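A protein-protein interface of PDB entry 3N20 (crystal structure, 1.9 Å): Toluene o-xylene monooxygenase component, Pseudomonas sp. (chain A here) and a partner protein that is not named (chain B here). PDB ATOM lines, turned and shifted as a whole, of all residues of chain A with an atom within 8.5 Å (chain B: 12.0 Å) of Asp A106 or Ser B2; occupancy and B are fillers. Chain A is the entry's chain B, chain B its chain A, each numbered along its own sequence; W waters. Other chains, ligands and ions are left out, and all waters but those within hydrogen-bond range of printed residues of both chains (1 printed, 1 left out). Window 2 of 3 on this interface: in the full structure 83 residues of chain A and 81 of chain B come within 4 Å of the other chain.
The backbone carbonyl oxygen (O) of Asp A102 lies within hydrogen-bond range of the backbone NH (N) of Ser B2 (2.8 Å). N of Ser B2 lies close to ND2 of Asn A105, 2.8 Å away. The side-chain carboxylate (OD2) of Asp A106 sits at hydrogen-bond distance from the backbone NH (N) of Ser B2 (2.8 Å). SD of Met B3 lies close to N of Asp A102, 3.7 Å away. SD of Met B3 lies close to OH of Tyr A171 (3.6 Å). The backbone NH (N) of Leu B4 is in hydrogen-bond range of the side-chain hydroxyl (OH) of Tyr A171, 2.9 Å away. O of Gln A98 sits close to SD of Met B3.
Tyr A171 touches Trp B9 (CD1 to CE2, 3.5 Å). Leu B4 touches Glu A175 (CD1 to CG, 3.7 Å).
Hydrophobic or aromatic side chains of chain A that line the printed part of chain B: Tyr A171. Along chain A the printed residues that touch a printed residue of chain B span positions 98 to 175. Printed residues of chain B that touch a printed residue of chain A: Ser B2, Met B3, Leu B4 and Trp B9. Hydrophobic or aromatic side chains of chain B within 4 Å of the printed part of chain A: Met B3, Leu B4 and Trp B9. Among the printed residues, 9 pairs touch across the chains. Among the printed residues, no Asp or Glu carboxylate lies within 4 Å of a Lys or Arg side-chain nitrogen of the other chain.
The guanidinium group (NH2) of Arg A172 is in salt-bridge range of the side-chain carboxylate (OE2) of Glu A175 (2.7 Å).
Water W1 bridges the side-chain amide nitrogen of Asn A105 (2.9 Å) and the side-chain hydroxyl of Ser B2 (3.5 Å).
Ser B2 touches just these residues of chain A: Asp A102, Asn A105 and Asp A106. Printed residues of chain B within 4 Å of Asp A102: Ser B2 (2.8 Å) and Met B3 (3.5 Å). Asn A105 touches just one residue of chain B: Ser B2. No residue of chain B comes within 4 Å of Gly A108. Printed residues of chain B within 4 Å of Tyr A171: Met B3, Leu B4 and Trp B9. Of the printed residues of chain A, Leu B4 touches Tyr A171 (2.9 Å) and Glu A175 (3.7 Å). Printed residues of chain A within 4 Å of Trp B9: Tyr A171 (3.5 Å). Of the printed residues of chain A, Met B3 touches Gln A98 (3.5 Å), Asp A102 (3.5 Å) and Tyr A171 (3.3 Å). Printed residues of chain B within 4 Å of Gln A98: Met B3. Gly A99 touches none of the printed residues of chain B. Arg A107 touches none of the printed residues of chain B. The nearest residue of chain A that does not touch Ser B2 is Phe A101 (4.1 Å). The nearest printed residue of chain A that does not touch Leu B4 is Arg A172 (5.7 Å).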
ATOM      1  N   GLN A  98     -23.458 -26.282 -19.930  1.00  0.00           N
ATOM      2  CA  GLN A  98     -22.056 -26.143 -19.555  1.00  0.00           C
ATOM      3  C   GLN A  98     -21.428 -27.538 -19.458  1.00  0.00           C
ATOM      4  O   GLN A  98     -20.219 -27.705 -19.643  1.00  0.00           O
ATOM      5  CB  GLN A  98     -21.923 -25.374 -18.231  1.00  0.00           C
ATOM      6  CG  GLN A  98     -22.653 -23.999 -18.181  1.00  0.00           C
ATOM      7  CD  GLN A  98     -22.233 -23.000 -19.275  1.00  0.00           C
ATOM      8  OE1 GLN A  98     -21.046 -22.696 -19.447  1.00  0.00           O
ATOM      9  NE2 GLN A  98     -23.220 -22.470 -20.001  1.00  0.00           N
ATOM     10  N   GLY A  99     -22.261 -28.540 -19.179  1.00  0.00           N
ATOM     11  CA  GLY A  99     -21.771 -29.904 -19.111  1.00  0.00           C
ATOM     12  C   GLY A  99     -21.377 -30.353 -20.511  1.00  0.00           C
ATOM     13  O   GLY A  99     -20.365 -31.029 -20.694  1.00  0.00           O
ATOM     14  N   LEU A 100     -22.182 -29.977 -21.504  1.00  0.00           N
ATOM     15  CA  LEU A 100     -21.900 -30.313 -22.901  1.00  0.00           C
ATOM     16  C   LEU A 100     -20.609 -29.651 -23.348  1.00  0.00           C
ATOM     17  O   LEU A 100     -19.758 -30.282 -23.976  1.00  0.00           O
ATOM     18  CB  LEU A 100     -23.022 -29.832 -23.822  1.00  0.00           C
ATOM     19  CG  LEU A 100     -24.245 -30.731 -23.996  1.00  0.00           C
ATOM     20  CD1 LEU A 100     -25.287 -30.026 -24.869  1.00  0.00           C
ATOM     21  CD2 LEU A 100     -23.814 -32.048 -24.635  1.00  0.00           C
ATOM     22  N   PHE A 101     -20.478 -28.366 -23.035  1.00  0.00           N
ATOM     23  CA  PHE A 101     -19.281 -27.621 -23.399  1.00  0.00           C
ATOM     24  C   PHE A 101     -18.058 -28.307 -22.819  1.00  0.00           C
ATOM     25  O   PHE A 101     -17.100 -28.592 -23.530  1.00  0.00           O
ATOM     26  CB  PHE A 101     -19.332 -26.189 -22.849  1.00  0.00           C
ATOM     27  CG  PHE A 101     -20.335 -25.296 -23.530  1.00  0.00           C
ATOM     28  CD1 PHE A 101     -20.454 -23.961 -23.147  1.00  0.00           C
ATOM     29  CD2 PHE A 101     -21.157 -25.777 -24.548  1.00  0.00           C
ATOM     30  CE1 PHE A 101     -21.374 -23.118 -23.767  1.00  0.00           C
ATOM     31  CE2 PHE A 101     -22.079 -24.941 -25.174  1.00  0.00           C
ATOM     32  CZ  PHE A 101     -22.187 -23.608 -24.782  1.00  0.00           C
ATOM     33  N   ASP A 102     -18.110 -28.572 -21.522  1.00  0.00           N
ATOM     34  CA  ASP A 102     -17.001 -29.186 -20.810  1.00  0.00           C
ATOM     35  C   ASP A 102     -16.596 -30.562 -21.327  1.00  0.00           C
ATOM     36  O   ASP A 102     -15.417 -30.819 -21.593  1.00  0.00           O
ATOM     37  CB  ASP A 102     -17.348 -29.258 -19.317  1.00  0.00           C
ATOM     38  CG  ASP A 102     -16.236 -29.854 -18.480  1.00  0.00           C
ATOM     39  OD1 ASP A 102     -15.051 -29.625 -18.802  1.00  0.00           O
ATOM     40  OD2 ASP A 102     -16.551 -30.539 -17.482  1.00  0.00           O
ATOM     41  N   GLN A 103     -17.575 -31.441 -21.497  1.00  0.00           N
ATOM     42  CA  GLN A 103     -17.275 -32.788 -21.933  1.00  0.00           C
ATOM     43  C   GLN A 103     -17.052 -33.005 -23.425  1.00  0.00           C
ATOM     44  O   GLN A 103     -16.314 -33.907 -23.801  1.00  0.00           O
ATOM     45  CB  GLN A 103     -18.324 -33.738 -21.334  1.00  0.00           C
ATOM     46  CG  GLN A 103     -18.162 -33.752 -19.799  1.00  0.00           C
ATOM     47  CD  GLN A 103     -19.033 -34.746 -19.073  1.00  0.00           C
ATOM     48  OE1 GLN A 103     -19.045 -35.936 -19.393  1.00  0.00           O
ATOM     49  NE2 GLN A 103     -19.754 -34.266 -18.057  1.00  0.00           N
ATOM     50  N   LEU A 104     -17.653 -32.188 -24.284  1.00  0.00           N
ATOM     51  CA  LEU A 104     -17.406 -32.357 -25.712  1.00  0.00           C
ATOM     52  C   LEU A 104     -16.014 -31.789 -26.006  1.00  0.00           C
ATOM     53  O   LEU A 104     -15.346 -32.198 -26.955  1.00  0.00           O
ATOM     54  CB  LEU A 104     -18.485 -31.659 -26.544  1.00  0.00           C
ATOM     55  CG  LEU A 104     -19.785 -32.473 -26.639  1.00  0.00           C
ATOM     56  CD1 LEU A 104     -20.861 -31.679 -27.373  1.00  0.00           C
ATOM     57  CD2 LEU A 104     -19.507 -33.784 -27.359  1.00  0.00           C
ATOM     58  N   ASN A 105     -15.574 -30.859 -25.167  1.00  0.00           N
ATOM     59  CA  ASN A 105     -14.249 -30.275 -25.308  1.00  0.00           C
ATOM     60  C   ASN A 105     -13.219 -31.340 -24.913  1.00  0.00           C
ATOM     61  O   ASN A 105     -12.224 -31.547 -25.613  1.00  0.00           O
ATOM     62  CB  ASN A 105     -14.098 -29.067 -24.390  1.00  0.00           C
ATOM     63  CG  ASN A 105     -12.671 -28.576 -24.316  1.00  0.00           C
ATOM     64  OD1 ASN A 105     -12.194 -27.881 -25.213  1.00  0.00           O
ATOM     65  ND2 ASN A 105     -11.971 -28.953 -23.258  1.00  0.00           N
ATOM     66  N   ASP A 106     -13.463 -32.007 -23.787  1.00  0.00           N
ATOM     67  CA  ASP A 106     -12.571 -33.063 -23.302  1.00  0.00           C
ATOM     68  C   ASP A 106     -12.400 -34.087 -24.406  1.00  0.00           C
ATOM     69  O   ASP A 106     -11.354 -34.717 -24.542  1.00  0.00           O
ATOM     70  CB  ASP A 106     -13.176 -33.764 -22.080  1.00  0.00           C
ATOM     71  CG  ASP A 106     -12.866 -33.057 -20.775  1.00  0.00           C
ATOM     72  OD1 ASP A 106     -13.558 -33.349 -19.775  1.00  0.00           O
ATOM     73  OD2 ASP A 106     -11.929 -32.228 -20.737  1.00  0.00           O
ATOM     74  N   ARG A 107     -13.453 -34.233 -25.197  1.00  0.00           N
ATOM     75  CA  ARG A 107     -13.493 -35.190 -26.289  1.00  0.00           C
ATOM     76  C   ARG A 107     -12.836 -34.711 -27.583  1.00  0.00           C
ATOM     77  O   ARG A 107     -12.652 -35.497 -28.507  1.00  0.00           O
ATOM     78  CB  ARG A 107     -14.949 -35.557 -26.557  1.00  0.00           C
ATOM     79  CG  ARG A 107     -15.123 -36.889 -27.218  1.00  0.00           C
ATOM     80  CD  ARG A 107     -16.415 -37.549 -26.763  1.00  0.00           C
ATOM     81  NE  ARG A 107     -17.532 -37.263 -27.650  1.00  0.00           N
ATOM     82  CZ  ARG A 107     -18.671 -37.949 -27.644  1.00  0.00           C
ATOM     83  NH1 ARG A 107     -19.644 -37.634 -28.490  1.00  0.00           N
ATOM     84  NH2 ARG A 107     -18.830 -38.954 -26.792  1.00  0.00           N
ATOM     85  N   GLY A 108     -12.485 -33.431 -27.652  1.00  0.00           N
ATOM     86  CA  GLY A 108     -11.868 -32.905 -28.860  1.00  0.00           C
ATOM     87  C   GLY A 108     -12.873 -32.758 -29.992  1.00  0.00           C
ATOM     88  O   GLY A 108     -12.532 -32.913 -31.167  1.00  0.00           O
ATOM     89  N   HIS A 109     -14.115 -32.445 -29.629  1.00  0.00           N
ATOM     90  CA  HIS A 109     -15.207 -32.277 -30.588  1.00  0.00           C
ATOM     91  C   HIS A 109     -14.949 -31.259 -31.707  1.00  0.00           C
ATOM     92  O   HIS A 109     -15.275 -31.513 -32.868  1.00  0.00           O
ATOM     93  CB  HIS A 109     -16.492 -31.907 -29.833  1.00  0.00           C
ATOM     94  CG  HIS A 109     -17.598 -31.410 -30.715  1.00  0.00           C
ATOM     95  ND1 HIS A 109     -17.609 -30.139 -31.254  1.00  0.00           N
ATOM     96  CD2 HIS A 109     -18.724 -32.017 -31.160  1.00  0.00           C
ATOM     97  CE1 HIS A 109     -18.692 -29.986 -31.995  1.00  0.00           C
ATOM     98  NE2 HIS A 109     -19.386 -31.110 -31.955  1.00  0.00           N
ATOM     99  N   ASP A 110     -14.370 -30.112 -31.369  1.00  0.00           N
ATOM    100  CA  ASP A 110     -14.115 -29.089 -32.377  1.00  0.00           C
ATOM    101  C   ASP A 110     -13.039 -29.480 -33.389  1.00  0.00           C
ATOM    102  O   ASP A 110     -13.086 -29.040 -34.539  1.00  0.00           O
ATOM    103  CB  ASP A 110     -13.769 -27.760 -31.698  1.00  0.00           C
ATOM    104  CG  ASP A 110     -14.953 -27.176 -30.934  1.00  0.00           C
ATOM    105  OD1 ASP A 110     -14.763 -26.175 -30.211  1.00  0.00           O
ATOM    106  OD2 ASP A 110     -16.076 -27.722 -31.058  1.00  0.00           O
ATOM    107  N   GLN A 111     -12.085 -30.312 -32.974  1.00  0.00           N
ATOM    108  CA  GLN A 111     -11.022 -30.765 -33.873  1.00  0.00           C
ATOM    109  C   GLN A 111     -11.543 -31.752 -34.909  1.00  0.00           C
ATOM    110  O   GLN A 111     -10.890 -31.997 -35.921  1.00  0.00           O
ATOM    111  CB  GLN A 111      -9.883 -31.423 -33.090  1.00  0.00           C
ATOM    112  CG  GLN A 111      -9.028 -30.441 -32.322  1.00  0.00           C
ATOM    113  CD  GLN A 111      -9.127 -30.637 -30.828  1.00  0.00           C
ATOM    114  OE1 GLN A 111      -8.383 -31.426 -30.240  1.00  0.00           O
ATOM    115  NE2 GLN A 111     -10.064 -29.928 -30.202  1.00  0.00           N
ATOM    116  N   TYR A 171     -19.033 -17.519 -25.714  1.00  0.00           N
ATOM    117  CA  TYR A 171     -18.184 -18.591 -25.201  1.00  0.00           C
ATOM    118  C   TYR A 171     -17.680 -19.502 -26.314  1.00  0.00           C
ATOM    119  O   TYR A 171     -16.478 -19.756 -26.431  1.00  0.00           O
ATOM    120  CB  TYR A 171     -18.954 -19.436 -24.183  1.00  0.00           C
ATOM    121  CG  TYR A 171     -18.106 -20.493 -23.507  1.00  0.00           C
ATOM    122  CD1 TYR A 171     -17.399 -20.202 -22.340  1.00  0.00           C
ATOM    123  CD2 TYR A 171     -17.995 -21.780 -24.046  1.00  0.00           C
ATOM    124  CE1 TYR A 171     -16.604 -21.166 -21.724  1.00  0.00           C
ATOM    125  CE2 TYR A 171     -17.200 -22.749 -23.438  1.00  0.00           C
ATOM    126  CZ  TYR A 171     -16.507 -22.436 -22.277  1.00  0.00           C
ATOM    127  OH  TYR A 171     -15.709 -23.379 -21.666  1.00  0.00           O
ATOM    128  N   ARG A 172     -18.605 -19.997 -27.126  1.00  0.00           N
ATOM    129  CA  ARG A 172     -18.245 -20.883 -28.218  1.00  0.00           C
ATOM    130  C   ARG A 172     -17.358 -20.202 -29.250  1.00  0.00           C
ATOM    131  O   ARG A 172     -16.526 -20.852 -29.879  1.00  0.00           O
ATOM    132  CB  ARG A 172     -19.513 -21.430 -28.875  1.00  0.00           C
ATOM    133  CG  ARG A 172     -20.206 -22.468 -28.011  1.00  0.00           C
ATOM    134  CD  ARG A 172     -19.321 -23.690 -27.917  1.00  0.00           C
ATOM    135  NE  ARG A 172     -19.158 -24.294 -29.236  1.00  0.00           N
ATOM    136  CZ  ARG A 172     -18.124 -25.042 -29.600  1.00  0.00           C
ATOM    137  NH1 ARG A 172     -18.079 -25.547 -30.825  1.00  0.00           N
ATOM    138  NH2 ARG A 172     -17.128 -25.269 -28.750  1.00  0.00           N
ATOM    139  N   GLU A 175     -13.870 -20.425 -27.991  1.00  0.00           N
ATOM    140  CA  GLU A 175     -13.434 -21.814 -28.104  1.00  0.00           C
ATOM    141  C   GLU A 175     -13.064 -22.128 -29.545  1.00  0.00           C
ATOM    142  O   GLU A 175     -12.063 -22.791 -29.809  1.00  0.00           O
ATOM    143  CB  GLU A 175     -14.537 -22.786 -27.662  1.00  0.00           C
ATOM    144  CG  GLU A 175     -14.668 -22.981 -26.171  1.00  0.00           C
ATOM    145  CD  GLU A 175     -15.178 -24.375 -25.826  1.00  0.00           C
ATOM    146  OE1 GLU A 175     -14.452 -25.123 -25.136  1.00  0.00           O
ATOM    147  OE2 GLU A 175     -16.300 -24.730 -26.251  1.00  0.00           O
ATOM    148  N   SER B   2     -12.956 -29.654 -20.764  1.00  0.00           N
ATOM    149  CA  SER B   2     -12.433 -28.505 -19.972  1.00  0.00           C
ATOM    150  C   SER B   2     -13.216 -27.231 -20.280  1.00  0.00           C
ATOM    151  O   SER B   2     -13.930 -27.164 -21.281  1.00  0.00           O
ATOM    152  CB  SER B   2     -10.950 -28.286 -20.285  1.00  0.00           C
ATOM    153  OG  SER B   2     -10.185 -29.422 -19.927  1.00  0.00           O
ATOM    154  N   MET B   3     -13.073 -26.231 -19.411  1.00  0.00           N
ATOM    155  CA  MET B   3     -13.756 -24.946 -19.569  1.00  0.00           C
ATOM    156  C   MET B   3     -12.743 -23.810 -19.720  1.00  0.00           C
ATOM    157  O   MET B   3     -11.614 -23.903 -19.229  1.00  0.00           O
ATOM    158  CB  MET B   3     -14.629 -24.641 -18.341  1.00  0.00           C
ATOM    159  CG  MET B   3     -15.709 -25.670 -18.015  1.00  0.00           C
ATOM    160  SD  MET B   3     -16.949 -25.811 -19.301  1.00  0.00           S
ATOM    161  CE  MET B   3     -17.947 -24.351 -18.999  1.00  0.00           C
ATOM    162  N   LEU B   4     -13.157 -22.738 -20.390  1.00  0.00           N
ATOM    163  CA  LEU B   4     -12.309 -21.559 -20.574  1.00  0.00           C
ATOM    164  C   LEU B   4     -12.323 -20.746 -19.286  1.00  0.00           C
ATOM    165  O   LEU B   4     -13.218 -20.904 -18.456  1.00  0.00           O
ATOM    166  CB  LEU B   4     -12.861 -20.663 -21.687  1.00  0.00           C
ATOM    167  CG  LEU B   4     -12.966 -21.162 -23.126  1.00  0.00           C
ATOM    168  CD1 LEU B   4     -13.856 -20.212 -23.935  1.00  0.00           C
ATOM    169  CD2 LEU B   4     -11.575 -21.262 -23.726  1.00  0.00           C
ATOM    170  N   LYS B   5     -11.328 -19.879 -19.121  1.00  0.00           N
ATOM    171  CA  LYS B   5     -11.267 -18.991 -17.965  1.00  0.00           C
ATOM    172  C   LYS B   5     -12.165 -17.829 -18.369  1.00  0.00           C
ATOM    173  O   LYS B   5     -12.151 -17.421 -19.525  1.00  0.00           O
ATOM    174  CB  LYS B   5      -9.828 -18.508 -17.731  1.00  0.00           C
ATOM    175  CG  LYS B   5      -9.011 -19.434 -16.831  1.00  0.00           C
ATOM    176  CD  LYS B   5      -7.614 -19.734 -17.375  1.00  0.00           C
ATOM    177  CE  LYS B   5      -6.638 -18.577 -17.189  1.00  0.00           C
ATOM    178  NZ  LYS B   5      -6.845 -17.457 -18.154  1.00  0.00           N
ATOM    179  N   ARG B   6     -12.954 -17.307 -17.436  1.00  0.00           N
ATOM    180  CA  ARG B   6     -13.864 -16.212 -17.755  1.00  0.00           C
ATOM    181  C   ARG B   6     -13.207 -15.066 -18.510  1.00  0.00           C
ATOM    182  O   ARG B   6     -13.745 -14.576 -19.504  1.00  0.00           O
ATOM    183  CB  ARG B   6     -14.515 -15.647 -16.488  1.00  0.00           C
ATOM    184  CG  ARG B   6     -15.580 -14.586 -16.797  1.00  0.00           C
ATOM    185  CD  ARG B   6     -16.289 -14.085 -15.549  1.00  0.00           C
ATOM    186  NE  ARG B   6     -15.443 -13.222 -14.734  1.00  0.00           N
ATOM    187  CZ  ARG B   6     -15.721 -12.882 -13.481  1.00  0.00           C
ATOM    188  NH1 ARG B   6     -16.824 -13.337 -12.900  1.00  0.00           N
ATOM    189  NH2 ARG B   6     -14.904 -12.082 -12.809  1.00  0.00           N
ATOM    190  N   ASP B   8     -10.866 -14.975 -20.561  1.00  0.00           N
ATOM    191  CA  ASP B   8     -10.510 -15.239 -21.950  1.00  0.00           C
ATOM    192  C   ASP B   8     -11.619 -15.009 -22.972  1.00  0.00           C
ATOM    193  O   ASP B   8     -11.339 -14.831 -24.155  1.00  0.00           O
ATOM    194  CB  ASP B   8      -9.966 -16.664 -22.096  1.00  0.00           C
ATOM    195  CG  ASP B   8      -8.646 -16.860 -21.366  1.00  0.00           C
ATOM    196  OD1 ASP B   8      -7.896 -15.868 -21.206  1.00  0.00           O
ATOM    197  OD2 ASP B   8      -8.348 -18.005 -20.965  1.00  0.00           O
ATOM    198  N   TRP B   9     -12.874 -15.001 -22.530  1.00  0.00           N
ATOM    199  CA  TRP B   9     -13.978 -14.794 -23.465  1.00  0.00           C
ATOM    200  C   TRP B   9     -14.952 -13.702 -23.050  1.00  0.00           C
ATOM    201  O   TRP B   9     -15.858 -13.358 -23.805  1.00  0.00           O
ATOM    202  CB  TRP B   9     -14.762 -16.097 -23.657  1.00  0.00           C
ATOM    203  CG  TRP B   9     -15.370 -16.640 -22.386  1.00  0.00           C
ATOM    204  CD1 TRP B   9     -14.732 -17.348 -21.409  1.00  0.00           C
ATOM    205  CD2 TRP B   9     -16.738 -16.527 -21.970  1.00  0.00           C
ATOM    206  NE1 TRP B   9     -15.616 -17.689 -20.412  1.00  0.00           N
ATOM    207  CE2 TRP B   9     -16.854 -17.199 -20.731  1.00  0.00           C
ATOM    208  CE3 TRP B   9     -17.879 -15.927 -22.525  1.00  0.00           C
ATOM    209  CZ2 TRP B   9     -18.071 -17.290 -20.036  1.00  0.00           C
ATOM    210  CZ3 TRP B   9     -19.090 -16.017 -21.832  1.00  0.00           C
ATOM    211  CH2 TRP B   9     -19.172 -16.695 -20.599  1.00  0.00           C
HETATM  212  O   HOH W   1      -9.315 -29.997 -23.257  1.00  0.00           O
